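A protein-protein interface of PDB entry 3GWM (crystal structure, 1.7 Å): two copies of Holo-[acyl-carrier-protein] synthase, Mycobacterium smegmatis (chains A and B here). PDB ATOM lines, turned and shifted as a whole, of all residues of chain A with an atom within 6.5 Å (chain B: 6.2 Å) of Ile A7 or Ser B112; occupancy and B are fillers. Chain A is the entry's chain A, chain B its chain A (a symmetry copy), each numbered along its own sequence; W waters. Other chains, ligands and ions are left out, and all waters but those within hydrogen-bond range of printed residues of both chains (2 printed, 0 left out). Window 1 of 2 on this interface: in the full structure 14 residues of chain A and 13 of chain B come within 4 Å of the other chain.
Of the 13 printed residues of chain B, 6 touch a printed residue of chain A.
Hydrophobic or aromatic side chains of chain B within 4 Å of the printed part of chain A: His B110, Ala B121 and Val B123.
Along chain B the printed residues that touch a printed residue of chain A span positions 110 to 123.
Of the 14 printed residues of chain A, 6 touch a printed residue of chain B.
OD1 of Asp A8 lies within salt-bridge range of NZ of Lys A61 (3.7 Å).
N of Ala B121 lies within hydrogen-bond range of O of Thr B114 (2.9 Å).
N of Ala A122 lies within hydrogen-bond range of O of Asp A8 (3.0 Å).
The backbone carbonyl oxygen (O) of Gly A6 lies within hydrogen-bond range of the backbone NH (N) of Ala A124.
O of Ser B112 is in hydrogen-bond range of N of Val B123, 3.0 Å away.
The backbone carbonyl oxygen (O) of Ile A7 sits at hydrogen-bond distance from the side-chain amino group (NZ) of Lys A61, 2.9 Å away.
Among the printed residues, merely in contact across the chains: Gly A6 with Ser B112 (3.3 Å), Ile A7 with Thr B114 (3.5 Å), Val A5 with Ser B112 (3.6 Å), Lys A61 with Thr B114 (3.6 Å), Val A5 with His B110 (3.8 Å), Leu A9 with Ala B121 (3.8 Å), Ile A7 with Val B123 (3.9 Å) and Val A5 with Val B123 (3.96 Å).
Water W2 bridges the backbone carbonyl oxygen of Val A5 and the side-chain hydroxyl of Ser B112.
Water W1 lies within hydrogen-bond range of O of Leu A9, OG1 of Thr B114 and OD1 of Asp A8.
The backbone NH (N) of Ile A7 is in hydrogen-bond range of the side-chain hydroxyl (OG) of Ser B112 (2.9 Å).
The side-chain hydroxyl (OG1) of Thr B114 sits at hydrogen-bond distance from the side-chain carboxylate (OD1) of Asp A8.
The side-chain hydroxyl of Thr B114 lies within hydrogen-bond range of the backbone NH of Leu A9 (3.1 Å).
NZ of Lys A61 sits at hydrogen-bond distance from O of Leu B113.
Ile A7 touches Val B123, but with the chains exchanged Val A123 does not touch Ile B7 (7.0 Å).
Positions printed for both chains: 7, 8, 121, 122, 123 and 124.
Of the 12 pairs that touch across the chains among the printed residues, none has its exchanged pair printed and touching as well.
Of the printed residues of chain B, Ile A7 touches Ser B112 (2.9 Å), Thr B114 (3.5 Å) and Val B123 (3.9 Å).
Printed residues of chain A within 4 Å of Ser B112: Val A5, Gly A6 and Ile A7.
Printed residues of chain B within 4 Å of Asp A8: Thr B114 (3.4 Å).
Of the printed residues of chain A, Val B123 touches Val A5 and Ile A7.
Of the printed residues of chain A, Thr B114 touches Ile A7 (3.5 Å), Asp A8 (3.4 Å), Leu A9 (3.1 Å) and Lys A61 (3.6 Å).
Printed residues of chain B within 4 Å of Gly A6: Ser B112.
Printed residues of chain A within 4 Å of His B110: Val A5.
The nearest printed residue of chain B that does not touch Ile A7 is Leu B113 (4.01 Å).
The nearest printed residue of chain A that does not touch Ser B112 is Lys A61 (4.01 Å).
The nearest printed residue of chain A that does not touch Leu B113 is Ile A7 (4.01 Å).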
ATOM      1  N   VAL A   5       0.319 -10.276 -13.655  1.00  0.00           N
ATOM      2  CA  VAL A   5      -1.012 -10.318 -13.045  1.00  0.00           C
ATOM      3  C   VAL A   5      -0.865 -10.341 -11.525  1.00  0.00           C
ATOM      4  O   VAL A   5       0.032 -10.989 -10.995  1.00  0.00           O
ATOM      5  CB  VAL A   5      -1.799 -11.565 -13.485  1.00  0.00           C
ATOM      6  CG1 VAL A   5      -3.194 -11.554 -12.881  1.00  0.00           C
ATOM      7  CG2 VAL A   5      -1.897 -11.626 -15.020  1.00  0.00           C
ATOM      8  N   GLY A   6      -1.742  -9.622 -10.830  1.00  0.00           N
ATOM      9  CA  GLY A   6      -1.694  -9.578  -9.382  1.00  0.00           C
ATOM     10  C   GLY A   6      -3.091  -9.507  -8.805  1.00  0.00           C
ATOM     11  O   GLY A   6      -3.969  -8.857  -9.346  1.00  0.00           O
ATOM     12  N   ILE A   7      -3.301 -10.194  -7.693  1.00  0.00           N
ATOM     13  CA  ILE A   7      -4.552 -10.075  -6.963  1.00  0.00           C
ATOM     14  C   ILE A   7      -4.169  -9.851  -5.514  1.00  0.00           C
ATOM     15  O   ILE A   7      -3.148 -10.361  -5.066  1.00  0.00           O
ATOM     16  CB  ILE A   7      -5.438 -11.330  -7.129  1.00  0.00           C
ATOM     17  CG1 ILE A   7      -6.796 -11.106  -6.465  1.00  0.00           C
ATOM     18  CG2 ILE A   7      -4.747 -12.577  -6.583  1.00  0.00           C
ATOM     19  CD1 ILE A   7      -7.809 -12.254  -6.713  1.00  0.00           C
ATOM     20  N   ASP A   8      -4.946  -9.041  -4.804  1.00  0.00           N
ATOM     21  CA  ASP A   8      -4.654  -8.765  -3.404  1.00  0.00           C
ATOM     22  C   ASP A   8      -5.946  -8.665  -2.611  1.00  0.00           C
ATOM     23  O   ASP A   8      -6.922  -8.033  -3.055  1.00  0.00           O
ATOM     24  CB  ASP A   8      -3.846  -7.474  -3.236  1.00  0.00           C
ATOM     25  CG  ASP A   8      -3.161  -7.395  -1.877  1.00  0.00           C
ATOM     26  OD1 ASP A   8      -2.398  -8.327  -1.563  1.00  0.00           O
ATOM     27  OD2 ASP A   8      -3.393  -6.429  -1.114  1.00  0.00           O
ATOM     28  N   LEU A   9      -5.922  -9.292  -1.439  1.00  0.00           N
ATOM     29  CA  LEU A   9      -7.014  -9.276  -0.486  1.00  0.00           C
ATOM     30  C   LEU A   9      -6.505  -8.557   0.769  1.00  0.00           C
ATOM     31  O   LEU A   9      -5.393  -8.811   1.228  1.00  0.00           O
ATOM     32  CB  LEU A   9      -7.375 -10.716  -0.147  1.00  0.00           C
ATOM     33  CG  LEU A   9      -8.824 -11.141  -0.001  1.00  0.00           C
ATOM     34  CD1 LEU A   9      -9.713 -10.491  -1.012  1.00  0.00           C
ATOM     35  CD2 LEU A   9      -8.870 -12.660  -0.120  1.00  0.00           C
ATOM     36  N   ALA A  54      -5.253  -2.219  -1.548  1.00  0.00           N
ATOM     37  CA  ALA A  54      -5.333  -3.509  -2.216  1.00  0.00           C
ATOM     38  C   ALA A  54      -4.947  -3.331  -3.679  1.00  0.00           C
ATOM     39  O   ALA A  54      -4.228  -4.151  -4.237  1.00  0.00           O
ATOM     40  CB  ALA A  54      -6.751  -4.096  -2.087  1.00  0.00           C
ATOM     41  N   GLU A  57      -1.195  -2.704  -4.033  1.00  0.00           N
ATOM     42  CA  GLU A  57      -0.484  -3.954  -3.763  1.00  0.00           C
ATOM     43  C   GLU A  57      -0.622  -4.908  -4.950  1.00  0.00           C
ATOM     44  O   GLU A  57       0.332  -5.608  -5.311  1.00  0.00           O
ATOM     45  CB  GLU A  57      -1.035  -4.636  -2.506  1.00  0.00           C
ATOM     46  CG  GLU A  57      -0.722  -3.885  -1.217  1.00  0.00           C
ATOM     47  CD  GLU A  57       0.709  -4.077  -0.783  1.00  0.00           C
ATOM     48  OE1 GLU A  57       0.943  -4.893   0.135  1.00  0.00           O
ATOM     49  OE2 GLU A  57       1.596  -3.429  -1.369  1.00  0.00           O
ATOM     50  N   ALA A  58      -1.809  -4.946  -5.544  1.00  0.00           N
ATOM     51  CA  ALA A  58      -2.045  -5.808  -6.709  1.00  0.00           C
ATOM     52  C   ALA A  58      -1.189  -5.369  -7.907  1.00  0.00           C
ATOM     53  O   ALA A  58      -0.612  -6.203  -8.597  1.00  0.00           O
ATOM     54  CB  ALA A  58      -3.529  -5.831  -7.082  1.00  0.00           C
ATOM     55  N   LYS A  61       2.397  -6.377  -7.147  1.00  0.00           N
ATOM     56  CA  LYS A  61       2.553  -7.821  -7.307  1.00  0.00           C
ATOM     57  C   LYS A  61       2.623  -8.195  -8.789  1.00  0.00           C
ATOM     58  O   LYS A  61       3.431  -9.039  -9.197  1.00  0.00           O
ATOM     59  CB  LYS A  61       1.415  -8.556  -6.606  1.00  0.00           C
ATOM     60  CG  LYS A  61       1.533  -8.488  -5.089  1.00  0.00           C
ATOM     61  CD  LYS A  61       0.307  -9.044  -4.396  1.00  0.00           C
ATOM     62  CE  LYS A  61       0.207 -10.549  -4.561  1.00  0.00           C
ATOM     63  NZ  LYS A  61      -0.780 -11.039  -3.565  1.00  0.00           N
ATOM     64  N   ALA A  62       1.784  -7.564  -9.600  1.00  0.00           N
ATOM     65  CA  ALA A  62       1.819  -7.814 -11.043  1.00  0.00           C
ATOM     66  C   ALA A  62       3.191  -7.405 -11.598  1.00  0.00           C
ATOM     67  O   ALA A  62       3.752  -8.074 -12.462  1.00  0.00           O
ATOM     68  CB  ALA A  62       0.706  -7.045 -11.736  1.00  0.00           C
ATOM     69  N   ALA A 121     -10.529  -5.916  -1.983  1.00  0.00           N
ATOM     70  CA  ALA A 121      -9.762  -6.719  -2.934  1.00  0.00           C
ATOM     71  C   ALA A 121      -9.489  -5.924  -4.193  1.00  0.00           C
ATOM     72  O   ALA A 121     -10.190  -4.976  -4.493  1.00  0.00           O
ATOM     73  CB  ALA A 121     -10.527  -8.008  -3.294  1.00  0.00           C
ATOM     74  N   ALA A 122      -8.460  -6.320  -4.936  1.00  0.00           N
ATOM     75  CA  ALA A 122      -8.195  -5.677  -6.214  1.00  0.00           C
ATOM     76  C   ALA A 122      -7.495  -6.657  -7.121  1.00  0.00           C
ATOM     77  O   ALA A 122      -6.845  -7.588  -6.645  1.00  0.00           O
ATOM     78  CB  ALA A 122      -7.333  -4.452  -6.022  1.00  0.00           C
ATOM     79  N   VAL A 123      -7.636  -6.454  -8.430  1.00  0.00           N
ATOM     80  CA  VAL A 123      -6.838  -7.207  -9.381  1.00  0.00           C
ATOM     81  C   VAL A 123      -6.156  -6.216 -10.319  1.00  0.00           C
ATOM     82  O   VAL A 123      -6.699  -5.152 -10.619  1.00  0.00           O
ATOM     83  CB  VAL A 123      -7.717  -8.215 -10.163  1.00  0.00           C
ATOM     84  CG1 VAL A 123      -8.787  -7.493 -10.984  1.00  0.00           C
ATOM     85  CG2 VAL A 123      -6.843  -9.098 -11.054  1.00  0.00           C
ATOM     86  N   ALA A 124      -4.949  -6.550 -10.759  1.00  0.00           N
ATOM     87  CA  ALA A 124      -4.231  -5.714 -11.703  1.00  0.00           C
ATOM     88  C   ALA A 124      -3.700  -6.604 -12.815  1.00  0.00           C
ATOM     89  O   ALA A 124      -3.205  -7.701 -12.565  1.00  0.00           O
ATOM     90  CB  ALA A 124      -3.078  -4.992 -10.999  1.00  0.00           C
ATOM     91  N   ILE B   7     -11.187 -17.635 -11.017  1.00  0.00           N
ATOM     92  CA  ILE B   7     -10.935 -17.005  -9.731  1.00  0.00           C
ATOM     93  C   ILE B   7     -11.434 -17.982  -8.685  1.00  0.00           C
ATOM     94  O   ILE B   7     -12.395 -18.702  -8.931  1.00  0.00           O
ATOM     95  CB  ILE B   7     -11.640 -15.635  -9.611  1.00  0.00           C
ATOM     96  CG1 ILE B   7     -11.235 -14.949  -8.307  1.00  0.00           C
ATOM     97  CG2 ILE B   7     -13.157 -15.776  -9.722  1.00  0.00           C
ATOM     98  CD1 ILE B   7     -11.773 -13.501  -8.170  1.00  0.00           C
ATOM     99  N   ASP B   8     -10.747 -18.053  -7.551  1.00  0.00           N
ATOM    100  CA  ASP B   8     -11.150 -18.965  -6.489  1.00  0.00           C
ATOM    101  C   ASP B   8     -10.924 -18.321  -5.133  1.00  0.00           C
ATOM    102  O   ASP B   8      -9.875 -17.696  -4.888  1.00  0.00           O
ATOM    103  CB  ASP B   8     -10.388 -20.293  -6.562  1.00  0.00           C
ATOM    104  CG  ASP B   8     -11.080 -21.398  -5.773  1.00  0.00           C
ATOM    105  OD1 ASP B   8     -12.263 -21.658  -6.064  1.00  0.00           O
ATOM    106  OD2 ASP B   8     -10.468 -21.990  -4.856  1.00  0.00           O
ATOM    107  N   ALA B  55      -4.965 -21.226  -5.758  1.00  0.00           N
ATOM    108  CA  ALA B  55      -4.298 -21.020  -7.044  1.00  0.00           C
ATOM    109  C   ALA B  55      -4.503 -22.210  -7.978  1.00  0.00           C
ATOM    110  O   ALA B  55      -4.813 -22.032  -9.156  1.00  0.00           O
ATOM    111  CB  ALA B  55      -2.807 -20.758  -6.827  1.00  0.00           C
ATOM    112  N   PRO B  92       4.060 -17.693  -6.761  1.00  0.00           N
ATOM    113  CA  PRO B  92       3.550 -18.950  -7.325  1.00  0.00           C
ATOM    114  C   PRO B  92       4.191 -19.337  -8.658  1.00  0.00           C
ATOM    115  O   PRO B  92       4.484 -18.470  -9.479  1.00  0.00           O
ATOM    116  CB  PRO B  92       2.069 -18.663  -7.570  1.00  0.00           C
ATOM    117  CG  PRO B  92       1.919 -17.168  -7.550  1.00  0.00           C
ATOM    118  CD  PRO B  92       3.162 -16.551  -7.013  1.00  0.00           C
ATOM    119  N   HIS B 110      -0.929 -17.579 -16.338  1.00  0.00           N
ATOM    120  CA  HIS B 110      -0.585 -16.555 -15.358  1.00  0.00           C
ATOM    121  C   HIS B 110      -1.343 -16.834 -14.084  1.00  0.00           C
ATOM    122  O   HIS B 110      -2.521 -17.160 -14.135  1.00  0.00           O
ATOM    123  CB  HIS B 110      -1.015 -15.182 -15.870  1.00  0.00           C
ATOM    124  CG  HIS B 110      -0.495 -14.860 -17.231  1.00  0.00           C
ATOM    125  ND1 HIS B 110       0.755 -14.325 -17.438  1.00  0.00           N
ATOM    126  CD2 HIS B 110      -1.053 -14.999 -18.457  1.00  0.00           C
ATOM    127  CE1 HIS B 110       0.943 -14.136 -18.734  1.00  0.00           C
ATOM    128  NE2 HIS B 110      -0.138 -14.537 -19.375  1.00  0.00           N
ATOM    129  N   VAL B 111      -0.699 -16.691 -12.931  1.00  0.00           N
ATOM    130  CA  VAL B 111      -1.418 -16.935 -11.690  1.00  0.00           C
ATOM    131  C   VAL B 111      -0.946 -15.982 -10.608  1.00  0.00           C
ATOM    132  O   VAL B 111       0.211 -15.581 -10.596  1.00  0.00           O
ATOM    133  CB  VAL B 111      -1.243 -18.399 -11.228  1.00  0.00           C
ATOM    134  CG1 VAL B 111       0.193 -18.656 -10.801  1.00  0.00           C
ATOM    135  CG2 VAL B 111      -2.221 -18.722 -10.121  1.00  0.00           C
ATOM    136  N   SER B 112      -1.869 -15.565  -9.737  1.00  0.00           N
ATOM    137  CA  SER B 112      -1.504 -14.738  -8.584  1.00  0.00           C
ATOM    138  C   SER B 112      -2.321 -15.233  -7.409  1.00  0.00           C
ATOM    139  O   SER B 112      -3.459 -15.659  -7.589  1.00  0.00           O
ATOM    140  CB  SER B 112      -1.782 -13.242  -8.843  1.00  0.00           C
ATOM    141  OG  SER B 112      -1.400 -12.436  -7.716  1.00  0.00           O
ATOM    142  N   LEU B 113      -1.736 -15.212  -6.217  1.00  0.00           N
ATOM    143  CA  LEU B 113      -2.461 -15.651  -5.036  1.00  0.00           C
ATOM    144  C   LEU B 113      -2.309 -14.647  -3.896  1.00  0.00           C
ATOM    145  O   LEU B 113      -1.427 -13.795  -3.914  1.00  0.00           O
ATOM    146  CB  LEU B 113      -2.032 -17.066  -4.616  1.00  0.00           C
ATOM    147  CG  LEU B 113      -0.545 -17.395  -4.529  1.00  0.00           C
ATOM    148  CD1 LEU B 113       0.119 -16.542  -3.475  1.00  0.00           C
ATOM    149  CD2 LEU B 113      -0.347 -18.894  -4.221  1.00  0.00           C
ATOM    150  N   THR B 114      -3.185 -14.748  -2.907  1.00  0.00           N
ATOM    151  CA  THR B 114      -3.187 -13.782  -1.826  1.00  0.00           C
ATOM    152  C   THR B 114      -3.936 -14.376  -0.652  1.00  0.00           C
ATOM    153  O   THR B 114      -4.705 -15.316  -0.817  1.00  0.00           O
ATOM    154  CB  THR B 114      -3.864 -12.461  -2.297  1.00  0.00           C
ATOM    155  OG1 THR B 114      -3.748 -11.451  -1.288  1.00  0.00           O
ATOM    156  CG2 THR B 114      -5.349 -12.679  -2.638  1.00  0.00           C
ATOM    157  N   ALA B 121      -7.232 -16.348  -1.750  1.00  0.00           N
ATOM    158  CA  ALA B 121      -7.819 -16.178  -3.080  1.00  0.00           C
ATOM    159  C   ALA B 121      -6.746 -16.286  -4.144  1.00  0.00           C
ATOM    160  O   ALA B 121      -5.577 -16.088  -3.870  1.00  0.00           O
ATOM    161  CB  ALA B 121      -8.519 -14.810  -3.191  1.00  0.00           C
ATOM    162  N   ALA B 122      -7.153 -16.601  -5.369  1.00  0.00           N
ATOM    163  CA  ALA B 122      -6.203 -16.620  -6.471  1.00  0.00           C
ATOM    164  C   ALA B 122      -6.934 -16.328  -7.757  1.00  0.00           C
ATOM    165  O   ALA B 122      -8.138 -16.565  -7.852  1.00  0.00           O
ATOM    166  CB  ALA B 122      -5.525 -17.967  -6.561  1.00  0.00           C
ATOM    167  N   VAL B 123      -6.207 -15.805  -8.742  1.00  0.00           N
ATOM    168  CA  VAL B 123      -6.760 -15.683 -10.079  1.00  0.00           C
ATOM    169  C   VAL B 123      -5.786 -16.331 -11.057  1.00  0.00           C
ATOM    170  O   VAL B 123      -4.572 -16.314 -10.848  1.00  0.00           O
ATOM    171  CB  VAL B 123      -7.018 -14.198 -10.436  1.00  0.00           C
ATOM    172  CG1 VAL B 123      -5.716 -13.397 -10.441  1.00  0.00           C
ATOM    173  CG2 VAL B 123      -7.732 -14.096 -11.784  1.00  0.00           C
ATOM    174  N   ALA B 124      -6.319 -16.934 -12.113  1.00  0.00           N
ATOM    175  CA  ALA B 124      -5.488 -17.532 -13.141  1.00  0.00           C
ATOM    176  C   ALA B 124      -6.003 -17.073 -14.495  1.00  0.00           C
ATOM    177  O   ALA B 124      -7.210 -17.018 -14.726  1.00  0.00           O
ATOM    178  CB  ALA B 124      -5.538 -19.060 -13.040  1.00  0.00           C
HETATM  179  O   HOH W   1      -2.830  -9.904   1.404  1.00  0.00           O
HETATM  180  O   HOH W   2       1.117 -11.754  -8.700  1.00  0.00           O
